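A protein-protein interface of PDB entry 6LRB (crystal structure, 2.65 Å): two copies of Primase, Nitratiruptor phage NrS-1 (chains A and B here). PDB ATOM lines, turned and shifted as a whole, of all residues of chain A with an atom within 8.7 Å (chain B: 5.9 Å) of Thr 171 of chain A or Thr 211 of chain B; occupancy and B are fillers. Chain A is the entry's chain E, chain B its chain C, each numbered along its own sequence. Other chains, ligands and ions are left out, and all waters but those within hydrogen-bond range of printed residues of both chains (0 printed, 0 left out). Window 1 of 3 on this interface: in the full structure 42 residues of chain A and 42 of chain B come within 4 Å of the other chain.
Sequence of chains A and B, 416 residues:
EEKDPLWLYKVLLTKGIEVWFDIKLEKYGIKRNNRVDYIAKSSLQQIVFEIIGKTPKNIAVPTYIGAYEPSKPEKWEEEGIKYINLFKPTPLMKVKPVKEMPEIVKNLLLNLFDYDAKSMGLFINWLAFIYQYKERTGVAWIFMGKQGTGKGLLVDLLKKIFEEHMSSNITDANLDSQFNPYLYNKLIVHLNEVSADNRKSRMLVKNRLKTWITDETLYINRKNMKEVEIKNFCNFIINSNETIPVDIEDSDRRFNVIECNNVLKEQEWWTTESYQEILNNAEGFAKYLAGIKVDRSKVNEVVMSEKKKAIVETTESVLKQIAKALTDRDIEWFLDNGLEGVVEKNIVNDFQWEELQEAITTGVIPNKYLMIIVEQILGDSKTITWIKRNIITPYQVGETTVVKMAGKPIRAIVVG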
ATOM      1  N   SER A 167     -33.512  15.067  25.209  1.00  0.00           N
ATOM      2  CA  SER A 167     -32.290  15.827  25.045  1.00  0.00           C
ATOM      3  C   SER A 167     -31.154  14.967  25.504  1.00  0.00           C
ATOM      4  O   SER A 167     -31.263  14.305  26.535  1.00  0.00           O
ATOM      5  CB  SER A 167     -32.333  17.099  25.868  1.00  0.00           C
ATOM      6  OG  SER A 167     -33.474  17.838  25.500  1.00  0.00           O
ATOM      7  N   SER A 168     -30.044  15.033  24.778  1.00  0.00           N
ATOM      8  CA  SER A 168     -28.931  14.123  24.994  1.00  0.00           C
ATOM      9  C   SER A 168     -27.653  14.890  25.279  1.00  0.00           C
ATOM     10  O   SER A 168     -27.369  15.895  24.621  1.00  0.00           O
ATOM     11  CB  SER A 168     -28.753  13.251  23.764  1.00  0.00           C
ATOM     12  OG  SER A 168     -30.007  13.049  23.130  1.00  0.00           O
ATOM     13  N   ASN A 169     -26.931  14.435  26.300  1.00  0.00           N
ATOM     14  CA  ASN A 169     -25.553  14.821  26.564  1.00  0.00           C
ATOM     15  C   ASN A 169     -25.518  16.321  26.841  1.00  0.00           C
ATOM     16  O   ASN A 169     -24.646  17.040  26.340  1.00  0.00           O
ATOM     17  CB  ASN A 169     -24.600  14.468  25.400  1.00  0.00           C
ATOM     18  CG  ASN A 169     -24.614  12.993  25.022  1.00  0.00           C
ATOM     19  OD1 ASN A 169     -23.905  12.181  25.620  1.00  0.00           O
ATOM     20  ND2 ASN A 169     -25.362  12.650  23.975  1.00  0.00           N
ATOM     21  N   ILE A 170     -26.480  16.788  27.630  1.00  0.00           N
ATOM     22  CA  ILE A 170     -26.495  18.160  28.101  1.00  0.00           C
ATOM     23  C   ILE A 170     -25.410  18.284  29.174  1.00  0.00           C
ATOM     24  O   ILE A 170     -25.280  17.428  30.040  1.00  0.00           O
ATOM     25  CB  ILE A 170     -27.874  18.528  28.661  1.00  0.00           C
ATOM     26  CG1 ILE A 170     -28.960  18.419  27.581  1.00  0.00           C
ATOM     27  CG2 ILE A 170     -27.875  19.927  29.256  1.00  0.00           C
ATOM     28  CD1 ILE A 170     -28.758  19.258  26.334  1.00  0.00           C
ATOM     29  N   THR A 171     -24.622  19.348  29.086  1.00  0.00           N
ATOM     30  CA  THR A 171     -23.438  19.548  29.915  1.00  0.00           C
ATOM     31  C   THR A 171     -23.621  20.780  30.773  1.00  0.00           C
ATOM     32  O   THR A 171     -24.572  21.535  30.601  1.00  0.00           O
ATOM     33  CB  THR A 171     -22.204  19.798  29.045  1.00  0.00           C
ATOM     34  OG1 THR A 171     -22.444  20.931  28.194  1.00  0.00           O
ATOM     35  CG2 THR A 171     -21.899  18.579  28.174  1.00  0.00           C
ATOM     36  N   ASP A 172     -22.688  20.991  31.692  1.00  0.00           N
ATOM     37  CA  ASP A 172     -22.675  22.200  32.515  1.00  0.00           C
ATOM     38  C   ASP A 172     -22.711  23.455  31.649  1.00  0.00           C
ATOM     39  O   ASP A 172     -23.445  24.392  31.952  1.00  0.00           O
ATOM     40  CB  ASP A 172     -21.454  22.213  33.437  1.00  0.00           C
ATOM     41  CG  ASP A 172     -21.586  21.233  34.584  1.00  0.00           C
ATOM     42  OD1 ASP A 172     -22.148  20.131  34.384  1.00  0.00           O
ATOM     43  OD2 ASP A 172     -21.154  21.581  35.705  1.00  0.00           O
ATOM     44  N   ALA A 173     -21.935  23.446  30.566  1.00  0.00           N
ATOM     45  CA  ALA A 173     -21.895  24.546  29.579  1.00  0.00           C
ATOM     46  C   ALA A 173     -23.263  24.953  29.051  1.00  0.00           C
ATOM     47  O   ALA A 173     -23.628  26.113  29.075  1.00  0.00           O
ATOM     48  CB  ALA A 173     -21.021  24.133  28.418  1.00  0.00           C
ATOM     49  N   ASN A 174     -24.044  23.967  28.619  1.00  0.00           N
ATOM     50  CA  ASN A 174     -25.433  24.181  28.175  1.00  0.00           C
ATOM     51  C   ASN A 174     -26.280  24.862  29.220  1.00  0.00           C
ATOM     52  O   ASN A 174     -27.192  25.612  28.896  1.00  0.00           O
ATOM     53  CB  ASN A 174     -26.095  22.841  27.887  1.00  0.00           C
ATOM     54  CG  ASN A 174     -25.462  22.109  26.726  1.00  0.00           C
ATOM     55  OD1 ASN A 174     -24.618  21.238  26.916  1.00  0.00           O
ATOM     56  ND2 ASN A 174     -25.892  22.428  25.526  1.00  0.00           N
ATOM     57  N   LEU A 175     -26.030  24.557  30.479  1.00  0.00           N
ATOM     58  CA  LEU A 175     -26.811  25.173  31.574  1.00  0.00           C
ATOM     59  C   LEU A 175     -26.426  26.637  31.784  1.00  0.00           C
ATOM     60  O   LEU A 175     -27.281  27.485  32.015  1.00  0.00           O
ATOM     61  CB  LEU A 175     -26.678  24.374  32.888  1.00  0.00           C
ATOM     62  CG  LEU A 175     -27.528  23.100  33.147  1.00  0.00           C
ATOM     63  CD1 LEU A 175     -27.838  22.301  31.887  1.00  0.00           C
ATOM     64  CD2 LEU A 175     -26.868  22.198  34.206  1.00  0.00           C
ATOM     65  N   ASP A 176     -25.120  26.923  31.706  1.00  0.00           N
ATOM     66  CA  ASP A 176     -24.616  28.315  31.788  1.00  0.00           C
ATOM     67  C   ASP A 176     -25.079  29.177  30.624  1.00  0.00           C
ATOM     68  O   ASP A 176     -25.164  30.383  30.790  1.00  0.00           O
ATOM     69  CB  ASP A 176     -23.095  28.370  31.876  1.00  0.00           C
ATOM     70  CG  ASP A 176     -22.589  27.992  33.247  1.00  0.00           C
ATOM     71  OD1 ASP A 176     -23.135  28.541  34.233  1.00  0.00           O
ATOM     72  OD2 ASP A 176     -21.660  27.139  33.331  1.00  0.00           O
ATOM     73  N   SER A 177     -25.407  28.553  29.482  1.00  0.00           N
ATOM     74  CA  SER A 177     -26.123  29.234  28.436  1.00  0.00           C
ATOM     75  C   SER A 177     -27.401  29.814  28.996  1.00  0.00           C
ATOM     76  O   SER A 177     -28.102  29.193  29.846  1.00  0.00           O
ATOM     77  CB  SER A 177     -26.497  28.328  27.281  1.00  0.00           C
ATOM     78  OG  SER A 177     -27.516  28.937  26.475  1.00  0.00           O
ATOM     79  N   TYR A 182     -33.212  22.640  25.648  1.00  0.00           N
ATOM     80  CA  TYR A 182     -33.071  21.254  26.089  1.00  0.00           C
ATOM     81  C   TYR A 182     -34.100  20.840  27.127  1.00  0.00           C
ATOM     82  O   TYR A 182     -34.075  19.679  27.538  1.00  0.00           O
ATOM     83  CB  TYR A 182     -31.645  20.984  26.658  1.00  0.00           C
ATOM     84  CG  TYR A 182     -31.183  22.025  27.657  1.00  0.00           C
ATOM     85  CD1 TYR A 182     -31.660  22.036  28.965  1.00  0.00           C
ATOM     86  CD2 TYR A 182     -30.308  23.026  27.284  1.00  0.00           C
ATOM     87  CE1 TYR A 182     -31.236  22.999  29.886  1.00  0.00           C
ATOM     88  CE2 TYR A 182     -29.907  24.008  28.187  1.00  0.00           C
ATOM     89  CZ  TYR A 182     -30.369  23.981  29.481  1.00  0.00           C
ATOM     90  OH  TYR A 182     -29.952  24.953  30.342  1.00  0.00           O
ATOM     91  N   VAL A 189     -34.574  13.967  29.620  1.00  0.00           N
ATOM     92  CA  VAL A 189     -33.490  14.934  29.525  1.00  0.00           C
ATOM     93  C   VAL A 189     -32.232  14.320  30.139  1.00  0.00           C
ATOM     94  O   VAL A 189     -32.160  14.100  31.351  1.00  0.00           O
ATOM     95  CB  VAL A 189     -33.814  16.255  30.270  1.00  0.00           C
ATOM     96  CG1 VAL A 189     -32.715  17.289  30.053  1.00  0.00           C
ATOM     97  CG2 VAL A 189     -35.125  16.839  29.790  1.00  0.00           C
ATOM     98  N   HIS A 190     -31.276  14.012  29.276  1.00  0.00           N
ATOM     99  CA  HIS A 190     -30.077  13.340  29.676  1.00  0.00           C
ATOM    100  C   HIS A 190     -28.952  14.337  29.899  1.00  0.00           C
ATOM    101  O   HIS A 190     -28.738  15.195  29.052  1.00  0.00           O
ATOM    102  CB  HIS A 190     -29.666  12.327  28.603  1.00  0.00           C
ATOM    103  CG  HIS A 190     -28.295  11.782  28.812  1.00  0.00           C
ATOM    104  ND1 HIS A 190     -27.364  11.711  27.802  1.00  0.00           N
ATOM    105  CD2 HIS A 190     -27.671  11.356  29.932  1.00  0.00           C
ATOM    106  CE1 HIS A 190     -26.227  11.247  28.286  1.00  0.00           C
ATOM    107  NE2 HIS A 190     -26.394  11.006  29.574  1.00  0.00           N
ATOM    108  N   LEU A 191     -28.209  14.171  30.998  1.00  0.00           N
ATOM    109  CA  LEU A 191     -27.065  15.015  31.318  1.00  0.00           C
ATOM    110  C   LEU A 191     -25.780  14.240  31.479  1.00  0.00           C
ATOM    111  O   LEU A 191     -25.758  13.156  32.081  1.00  0.00           O
ATOM    112  CB  LEU A 191     -27.324  15.731  32.633  1.00  0.00           C
ATOM    113  CG  LEU A 191     -28.401  16.802  32.629  1.00  0.00           C
ATOM    114  CD1 LEU A 191     -28.903  17.096  34.020  1.00  0.00           C
ATOM    115  CD2 LEU A 191     -27.864  18.078  32.047  1.00  0.00           C
ATOM    116  N   ASN A 192     -24.688  14.812  31.004  1.00  0.00           N
ATOM    117  CA  ASN A 192     -23.331  14.227  31.202  1.00  0.00           C
ATOM    118  C   ASN A 192     -22.611  15.070  32.222  1.00  0.00           C
ATOM    119  O   ASN A 192     -22.482  16.311  32.028  1.00  0.00           O
ATOM    120  CB  ASN A 192     -22.496  14.271  29.913  1.00  0.00           C
ATOM    121  CG  ASN A 192     -22.472  12.960  29.185  1.00  0.00           C
ATOM    122  OD1 ASN A 192     -23.017  12.838  28.086  1.00  0.00           O
ATOM    123  ND2 ASN A 192     -21.807  11.977  29.762  1.00  0.00           N
ATOM    124  N   GLU A 193     -22.103  14.406  33.231  1.00  0.00           N
ATOM    125  CA  GLU A 193     -21.226  15.042  34.157  1.00  0.00           C
ATOM    126  C   GLU A 193     -19.869  14.719  33.588  1.00  0.00           C
ATOM    127  O   GLU A 193     -19.610  13.629  33.147  1.00  0.00           O
ATOM    128  CB  GLU A 193     -21.341  14.484  35.548  1.00  0.00           C
ATOM    129  CG  GLU A 193     -20.412  15.147  36.530  1.00  0.00           C
ATOM    130  CD  GLU A 193     -20.588  16.638  36.587  1.00  0.00           C
ATOM    131  OE1 GLU A 193     -19.777  17.342  36.004  1.00  0.00           O
ATOM    132  OE2 GLU A 193     -21.523  17.125  37.221  1.00  0.00           O
ATOM    133  N   VAL A 194     -19.012  15.701  33.500  1.00  0.00           N
ATOM    134  CA  VAL A 194     -17.705  15.435  32.971  1.00  0.00           C
ATOM    135  C   VAL A 194     -16.567  15.940  33.846  1.00  0.00           C
ATOM    136  O   VAL A 194     -15.438  15.594  33.664  1.00  0.00           O
ATOM    137  CB  VAL A 194     -17.620  15.917  31.533  1.00  0.00           C
ATOM    138  CG1 VAL A 194     -18.076  14.836  30.585  1.00  0.00           C
ATOM    139  CG2 VAL A 194     -18.412  17.176  31.356  1.00  0.00           C
ATOM    140  N   SER A 195     -16.890  16.687  34.875  1.00  0.00           N
ATOM    141  CA  SER A 195     -15.869  17.245  35.737  1.00  0.00           C
ATOM    142  C   SER A 195     -15.096  16.188  36.466  1.00  0.00           C
ATOM    143  O   SER A 195     -15.617  15.155  36.815  1.00  0.00           O
ATOM    144  CB  SER A 195     -16.490  18.199  36.755  1.00  0.00           C
ATOM    145  OG  SER A 195     -16.567  19.527  36.255  1.00  0.00           O
ATOM    146  N   VAL A 205     -23.055  22.698  39.858  1.00  0.00           N
ATOM    147  CA  VAL A 205     -24.151  23.519  39.227  1.00  0.00           C
ATOM    148  C   VAL A 205     -25.438  22.780  38.807  1.00  0.00           C
ATOM    149  O   VAL A 205     -26.446  23.421  38.499  1.00  0.00           O
ATOM    150  CB  VAL A 205     -23.689  24.377  37.981  1.00  0.00           C
ATOM    151  CG1 VAL A 205     -22.622  25.367  38.404  1.00  0.00           C
ATOM    152  CG2 VAL A 205     -23.179  23.521  36.818  1.00  0.00           C
ATOM    153  N   LYS A 206     -25.392  21.448  38.744  1.00  0.00           N
ATOM    154  CA  LYS A 206     -26.574  20.646  38.457  1.00  0.00           C
ATOM    155  C   LYS A 206     -27.546  20.533  39.625  1.00  0.00           C
ATOM    156  O   LYS A 206     -28.622  19.961  39.444  1.00  0.00           O
ATOM    157  CB  LYS A 206     -26.171  19.254  37.988  1.00  0.00           C
ATOM    158  CG  LYS A 206     -25.649  19.228  36.569  1.00  0.00           C
ATOM    159  CD  LYS A 206     -24.993  17.898  36.245  1.00  0.00           C
ATOM    160  CE  LYS A 206     -24.541  17.880  34.784  1.00  0.00           C
ATOM    161  NZ  LYS A 206     -23.084  17.621  34.687  1.00  0.00           N
ATOM    162  N   ARG A 208     -29.615  22.566  40.545  1.00  0.00           N
ATOM    163  CA  ARG A 208     -30.893  23.179  40.046  1.00  0.00           C
ATOM    164  C   ARG A 208     -31.852  22.158  39.484  1.00  0.00           C
ATOM    165  O   ARG A 208     -33.065  22.330  39.527  1.00  0.00           O
ATOM    166  CB  ARG A 208     -30.627  24.255  38.970  1.00  0.00           C
ATOM    167  CG  ARG A 208     -29.943  23.764  37.689  1.00  0.00           C
ATOM    168  CD  ARG A 208     -29.752  24.869  36.654  1.00  0.00           C
ATOM    169  NE  ARG A 208     -28.709  25.820  37.063  1.00  0.00           N
ATOM    170  CZ  ARG A 208     -28.083  26.703  36.273  1.00  0.00           C
ATOM    171  NH1 ARG A 208     -28.370  26.814  34.981  1.00  0.00           N
ATOM    172  NH2 ARG A 208     -27.148  27.499  36.794  1.00  0.00           N
ATOM    173  N   TRP A 212     -36.141  20.893  39.095  1.00  0.00           N
ATOM    174  CA  TRP A 212     -36.718  20.522  37.775  1.00  0.00           C
ATOM    175  C   TRP A 212     -37.455  19.169  37.771  1.00  0.00           C
ATOM    176  O   TRP A 212     -38.475  18.998  37.084  1.00  0.00           O
ATOM    177  CB  TRP A 212     -35.631  20.432  36.679  1.00  0.00           C
ATOM    178  CG  TRP A 212     -34.899  21.708  36.367  1.00  0.00           C
ATOM    179  CD1 TRP A 212     -35.251  22.973  36.743  1.00  0.00           C
ATOM    180  CD2 TRP A 212     -33.724  21.842  35.562  1.00  0.00           C
ATOM    181  NE1 TRP A 212     -34.343  23.877  36.260  1.00  0.00           N
ATOM    182  CE2 TRP A 212     -33.399  23.212  35.520  1.00  0.00           C
ATOM    183  CE3 TRP A 212     -32.902  20.932  34.880  1.00  0.00           C
ATOM    184  CZ2 TRP A 212     -32.286  23.701  34.820  1.00  0.00           C
ATOM    185  CZ3 TRP A 212     -31.779  21.421  34.186  1.00  0.00           C
ATOM    186  CH2 TRP A 212     -31.491  22.786  34.163  1.00  0.00           C
ATOM    187  N   ASN A 239     -25.573  10.686  33.353  1.00  0.00           N
ATOM    188  CA  ASN A 239     -24.457   9.817  33.257  1.00  0.00           C
ATOM    189  C   ASN A 239     -23.334  10.577  33.880  1.00  0.00           C
ATOM    190  O   ASN A 239     -23.205  11.759  33.729  1.00  0.00           O
ATOM    191  CB  ASN A 239     -24.142   9.495  31.822  1.00  0.00           C
ATOM    192  CG  ASN A 239     -25.080   8.487  31.257  1.00  0.00           C
ATOM    193  OD1 ASN A 239     -25.901   7.964  31.956  1.00  0.00           O
ATOM    194  ND2 ASN A 239     -24.972   8.227  29.985  1.00  0.00           N
ATOM    195  N   ASN B 207     -13.734  20.170  28.109  1.00  0.00           N
ATOM    196  CA  ASN B 207     -14.333  18.968  28.589  1.00  0.00           C
ATOM    197  C   ASN B 207     -15.720  18.752  28.033  1.00  0.00           C
ATOM    198  O   ASN B 207     -16.250  17.672  28.134  1.00  0.00           O
ATOM    199  CB  ASN B 207     -14.419  19.058  30.099  1.00  0.00           C
ATOM    200  CG  ASN B 207     -13.386  18.229  30.779  1.00  0.00           C
ATOM    201  OD1 ASN B 207     -13.489  17.029  30.783  1.00  0.00           O
ATOM    202  ND2 ASN B 207     -12.383  18.859  31.347  1.00  0.00           N
ATOM    203  N   ARG B 208     -16.274  19.891  27.654  1.00  0.00           N
ATOM    204  CA  ARG B 208     -17.557  20.015  27.020  1.00  0.00           C
ATOM    205  C   ARG B 208     -17.484  19.348  25.690  1.00  0.00           C
ATOM    206  O   ARG B 208     -18.458  18.881  25.172  1.00  0.00           O
ATOM    207  CB  ARG B 208     -17.940  21.472  26.856  1.00  0.00           C
ATOM    208  CG  ARG B 208     -17.044  22.312  25.981  1.00  0.00           C
ATOM    209  CD  ARG B 208     -17.627  23.691  25.818  1.00  0.00           C
ATOM    210  NE  ARG B 208     -17.617  24.400  27.079  1.00  0.00           N
ATOM    211  CZ  ARG B 208     -17.672  25.718  27.186  1.00  0.00           C
ATOM    212  NH1 ARG B 208     -17.740  26.460  26.102  1.00  0.00           N
ATOM    213  NH2 ARG B 208     -17.662  26.293  28.375  1.00  0.00           N
ATOM    214  N   LEU B 209     -16.284  19.304  25.138  1.00  0.00           N
ATOM    215  CA  LEU B 209     -16.065  18.679  23.851  1.00  0.00           C
ATOM    216  C   LEU B 209     -16.383  17.188  23.898  1.00  0.00           C
ATOM    217  O   LEU B 209     -16.901  16.626  22.933  1.00  0.00           O
ATOM    218  CB  LEU B 209     -14.621  18.892  23.391  1.00  0.00           C
ATOM    219  CG  LEU B 209     -13.960  17.718  22.667  1.00  0.00           C
ATOM    220  CD1 LEU B 209     -14.568  17.528  21.285  1.00  0.00           C
ATOM    221  CD2 LEU B 209     -12.456  17.925  22.571  1.00  0.00           C
ATOM    222  N   LYS B 210     -16.070  16.549  25.022  1.00  0.00           N
ATOM    223  CA  LYS B 210     -16.231  15.130  25.121  1.00  0.00           C
ATOM    224  C   LYS B 210     -17.604  14.706  24.668  1.00  0.00           C
ATOM    225  O   LYS B 210     -17.723  13.720  23.984  1.00  0.00           O
ATOM    226  CB  LYS B 210     -16.017  14.714  26.567  1.00  0.00           C
ATOM    227  CG  LYS B 210     -14.621  14.972  27.072  1.00  0.00           C
ATOM    228  CD  LYS B 210     -14.526  14.964  28.576  1.00  0.00           C
ATOM    229  CE  LYS B 210     -13.495  13.976  29.070  1.00  0.00           C
ATOM    230  NZ  LYS B 210     -13.580  13.712  30.515  1.00  0.00           N
ATOM    231  N   THR B 211     -18.648  15.406  25.055  1.00  0.00           N
ATOM    232  CA  THR B 211     -19.929  15.056  24.542  1.00  0.00           C
ATOM    233  C   THR B 211     -20.005  15.312  23.052  1.00  0.00           C
ATOM    234  O   THR B 211     -20.365  14.443  22.273  1.00  0.00           O
ATOM    235  CB  THR B 211     -20.963  15.947  25.184  1.00  0.00           C
ATOM    236  OG1 THR B 211     -20.903  17.248  24.586  1.00  0.00           O
ATOM    237  CG2 THR B 211     -20.659  16.063  26.628  1.00  0.00           C
ATOM    238  N   TRP B 212     -19.573  16.483  22.634  1.00  0.00           N
ATOM    239  CA  TRP B 212     -19.656  16.802  21.199  1.00  0.00           C
ATOM    240  C   TRP B 212     -19.214  15.636  20.291  1.00  0.00           C
ATOM    241  O   TRP B 212     -19.726  15.451  19.168  1.00  0.00           O
ATOM    242  CB  TRP B 212     -18.777  18.012  20.845  1.00  0.00           C
ATOM    243  CG  TRP B 212     -19.152  19.318  21.482  1.00  0.00           C
ATOM    244  CD1 TRP B 212     -20.311  19.611  22.127  1.00  0.00           C
ATOM    245  CD2 TRP B 212     -18.363  20.523  21.497  1.00  0.00           C
ATOM    246  NE1 TRP B 212     -20.294  20.922  22.563  1.00  0.00           N
ATOM    247  CE2 TRP B 212     -19.109  21.502  22.191  1.00  0.00           C
ATOM    248  CE3 TRP B 212     -17.089  20.860  21.012  1.00  0.00           C
ATOM    249  CZ2 TRP B 212     -18.629  22.799  22.409  1.00  0.00           C
ATOM    250  CZ3 TRP B 212     -16.611  22.161  21.230  1.00  0.00           C
ATOM    251  CH2 TRP B 212     -17.383  23.107  21.922  1.00  0.00           C
ATOM    252  N   ILE B 213     -18.210  14.898  20.750  1.00  0.00           N
ATOM    253  CA  ILE B 213     -17.625  13.775  19.999  1.00  0.00           C
ATOM    254  C   ILE B 213     -18.697  12.789  19.677  1.00  0.00           C
ATOM    255  O   ILE B 213     -18.736  12.247  18.574  1.00  0.00           O
ATOM    256  CB  ILE B 213     -16.510  13.117  20.826  1.00  0.00           C
ATOM    257  CG1 ILE B 213     -15.252  14.013  20.786  1.00  0.00           C
ATOM    258  CG2 ILE B 213     -16.152  11.726  20.334  1.00  0.00           C
ATOM    259  CD1 ILE B 213     -14.316  13.800  21.964  1.00  0.00           C
ATOM    260  N   THR B 214     -19.583  12.567  20.641  1.00  0.00           N
ATOM    261  CA  THR B 214     -20.564  11.472  20.585  1.00  0.00           C
ATOM    262  C   THR B 214     -22.026  11.898  20.502  1.00  0.00           C
ATOM    263  O   THR B 214     -22.888  11.038  20.313  1.00  0.00           O
ATOM    264  CB  THR B 214     -20.443  10.601  21.854  1.00  0.00           C
ATOM    265  OG1 THR B 214     -20.456  11.457  23.001  1.00  0.00           O
ATOM    266  CG2 THR B 214     -19.148   9.829  21.843  1.00  0.00           C
ATOM    267  N   ASP B 215     -22.317  13.191  20.622  1.00  0.00           N
ATOM    268  CA  ASP B 215     -23.709  13.638  20.611  1.00  0.00           C
ATOM    269  C   ASP B 215     -24.241  13.585  19.179  1.00  0.00           C
ATOM    270  O   ASP B 215     -23.577  14.049  18.250  1.00  0.00           O
ATOM    271  CB  ASP B 215     -23.854  15.046  21.203  1.00  0.00           C
ATOM    272  CG  ASP B 215     -25.298  15.396  21.578  1.00  0.00           C
ATOM    273  OD1 ASP B 215     -26.249  14.674  21.185  1.00  0.00           O
ATOM    274  OD2 ASP B 215     -25.491  16.438  22.245  1.00  0.00           O
ATOM    275  N   ASN B 232     -24.986  16.237  13.942  1.00  0.00           N
ATOM    276  CA  ASN B 232     -23.555  16.435  14.237  1.00  0.00           C
ATOM    277  C   ASN B 232     -22.653  15.578  13.372  1.00  0.00           C
ATOM    278  O   ASN B 232     -22.763  14.350  13.411  1.00  0.00           O
ATOM    279  CB  ASN B 232     -23.289  16.064  15.689  1.00  0.00           C
ATOM    280  CG  ASN B 232     -21.876  16.380  16.121  1.00  0.00           C
ATOM    281  OD1 ASN B 232     -21.112  17.035  15.385  1.00  0.00           O
ATOM    282  ND2 ASN B 232     -21.515  15.930  17.336  1.00  0.00           N
ATOM    283  N   ARG B 254     -12.953   7.669  24.126  1.00  0.00           N
ATOM    284  CA  ARG B 254     -13.057   8.769  23.148  1.00  0.00           C
ATOM    285  C   ARG B 254     -11.698   9.255  22.579  1.00  0.00           C
ATOM    286  O   ARG B 254     -11.620   9.711  21.440  1.00  0.00           O
ATOM    287  CB  ARG B 254     -13.789   9.953  23.792  1.00  0.00           C
ATOM    288  CG  ARG B 254     -15.321   9.875  23.820  1.00  0.00           C
ATOM    289  CD  ARG B 254     -15.835  10.169  25.224  1.00  0.00           C
ATOM    290  NE  ARG B 254     -17.284  10.384  25.402  1.00  0.00           N
ATOM    291  CZ  ARG B 254     -18.266   9.473  25.311  1.00  0.00           C
ATOM    292  NH1 ARG B 254     -18.031   8.208  24.963  1.00  0.00           N
ATOM    293  NH2 ARG B 254     -19.525   9.853  25.539  1.00  0.00           N
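O of Asp 215 of chain B is in hydrogen-bond range of ND2 of Asn 232 of chain B (2.9 Å).
O of Arg 208 of chain B sits at hydrogen-bond distance from OG1 of Thr 211 of chain B (3.0 Å).
The backbone NH (N) of Asn 169 of chain A sits at hydrogen-bond distance from a ring nitrogen (ND1) of His 190 of chain A, at 3.1 Å.
The side-chain amide oxygen of Asn 174 of chain A lies within hydrogen-bond range of the side-chain hydroxyl of Thr 171 of chain A, at 2.5 Å.
The side-chain amino group (NZ) of Lys 210 of chain B sits close to the side-chain amide oxygen (OD1) of Asn 207 of chain B, at 3.3 Å.
The side-chain amide oxygen (OD1) of Asn 169 of chain A lies close to the side-chain amide oxygen (OD1) of Asn 192 of chain A.
Positions printed for both chains: 208 and 212.
Of the 6 pairs that touch across the chains among the printed residues, none has its exchanged pair printed and touching as well.
O of Ser 168 of chain A sits close to OD2 of Asp 215 of chain B, 3.1 Å away.
Along chain A the printed residues that touch a printed residue of chain B span positions 168 to 194.
Of the 11 printed residues of chain B, 4 touch a printed residue of chain A.
Among the printed residues, 6 pairs touch across the chains.
Among the printed residues, pairs that only touch across the chains: Thr 171 of chain A with Thr 211 of chain B, Asn 169 of chain A with Asp 215 of chain B, Ala 173 of chain A with Arg 208 of chain B, Val 194 of chain A with Asn 207 of chain B and Asn 169 of chain A with Thr 211 of chain B.
Of chain A, only Asn 169 and Thr 171 come within 4 Å of Thr 211 of chain B.
Of the printed residues of chain B, Val 194 of chain A touches Asn 207.
Printed residues of chain B within 4 Å of Ser 168 of chain A: Asp 215 (3.1 Å).
Printed residues of chain A within 4 Å of Asp 215 of chain B: Ser 168 and Asn 169.
Printed residues of chain A within 4 Å of Arg 208 of chain B: Ala 173.
Of the printed residues of chain B, Ala 173 of chain A touches Arg 208 (3.7 Å).
Leu 175 of chain A touches none of the printed residues of chain B.
The nearest residue of chain A that does not touch Thr 211 of chain B is Asn 192 of chain A (4.2 Å).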
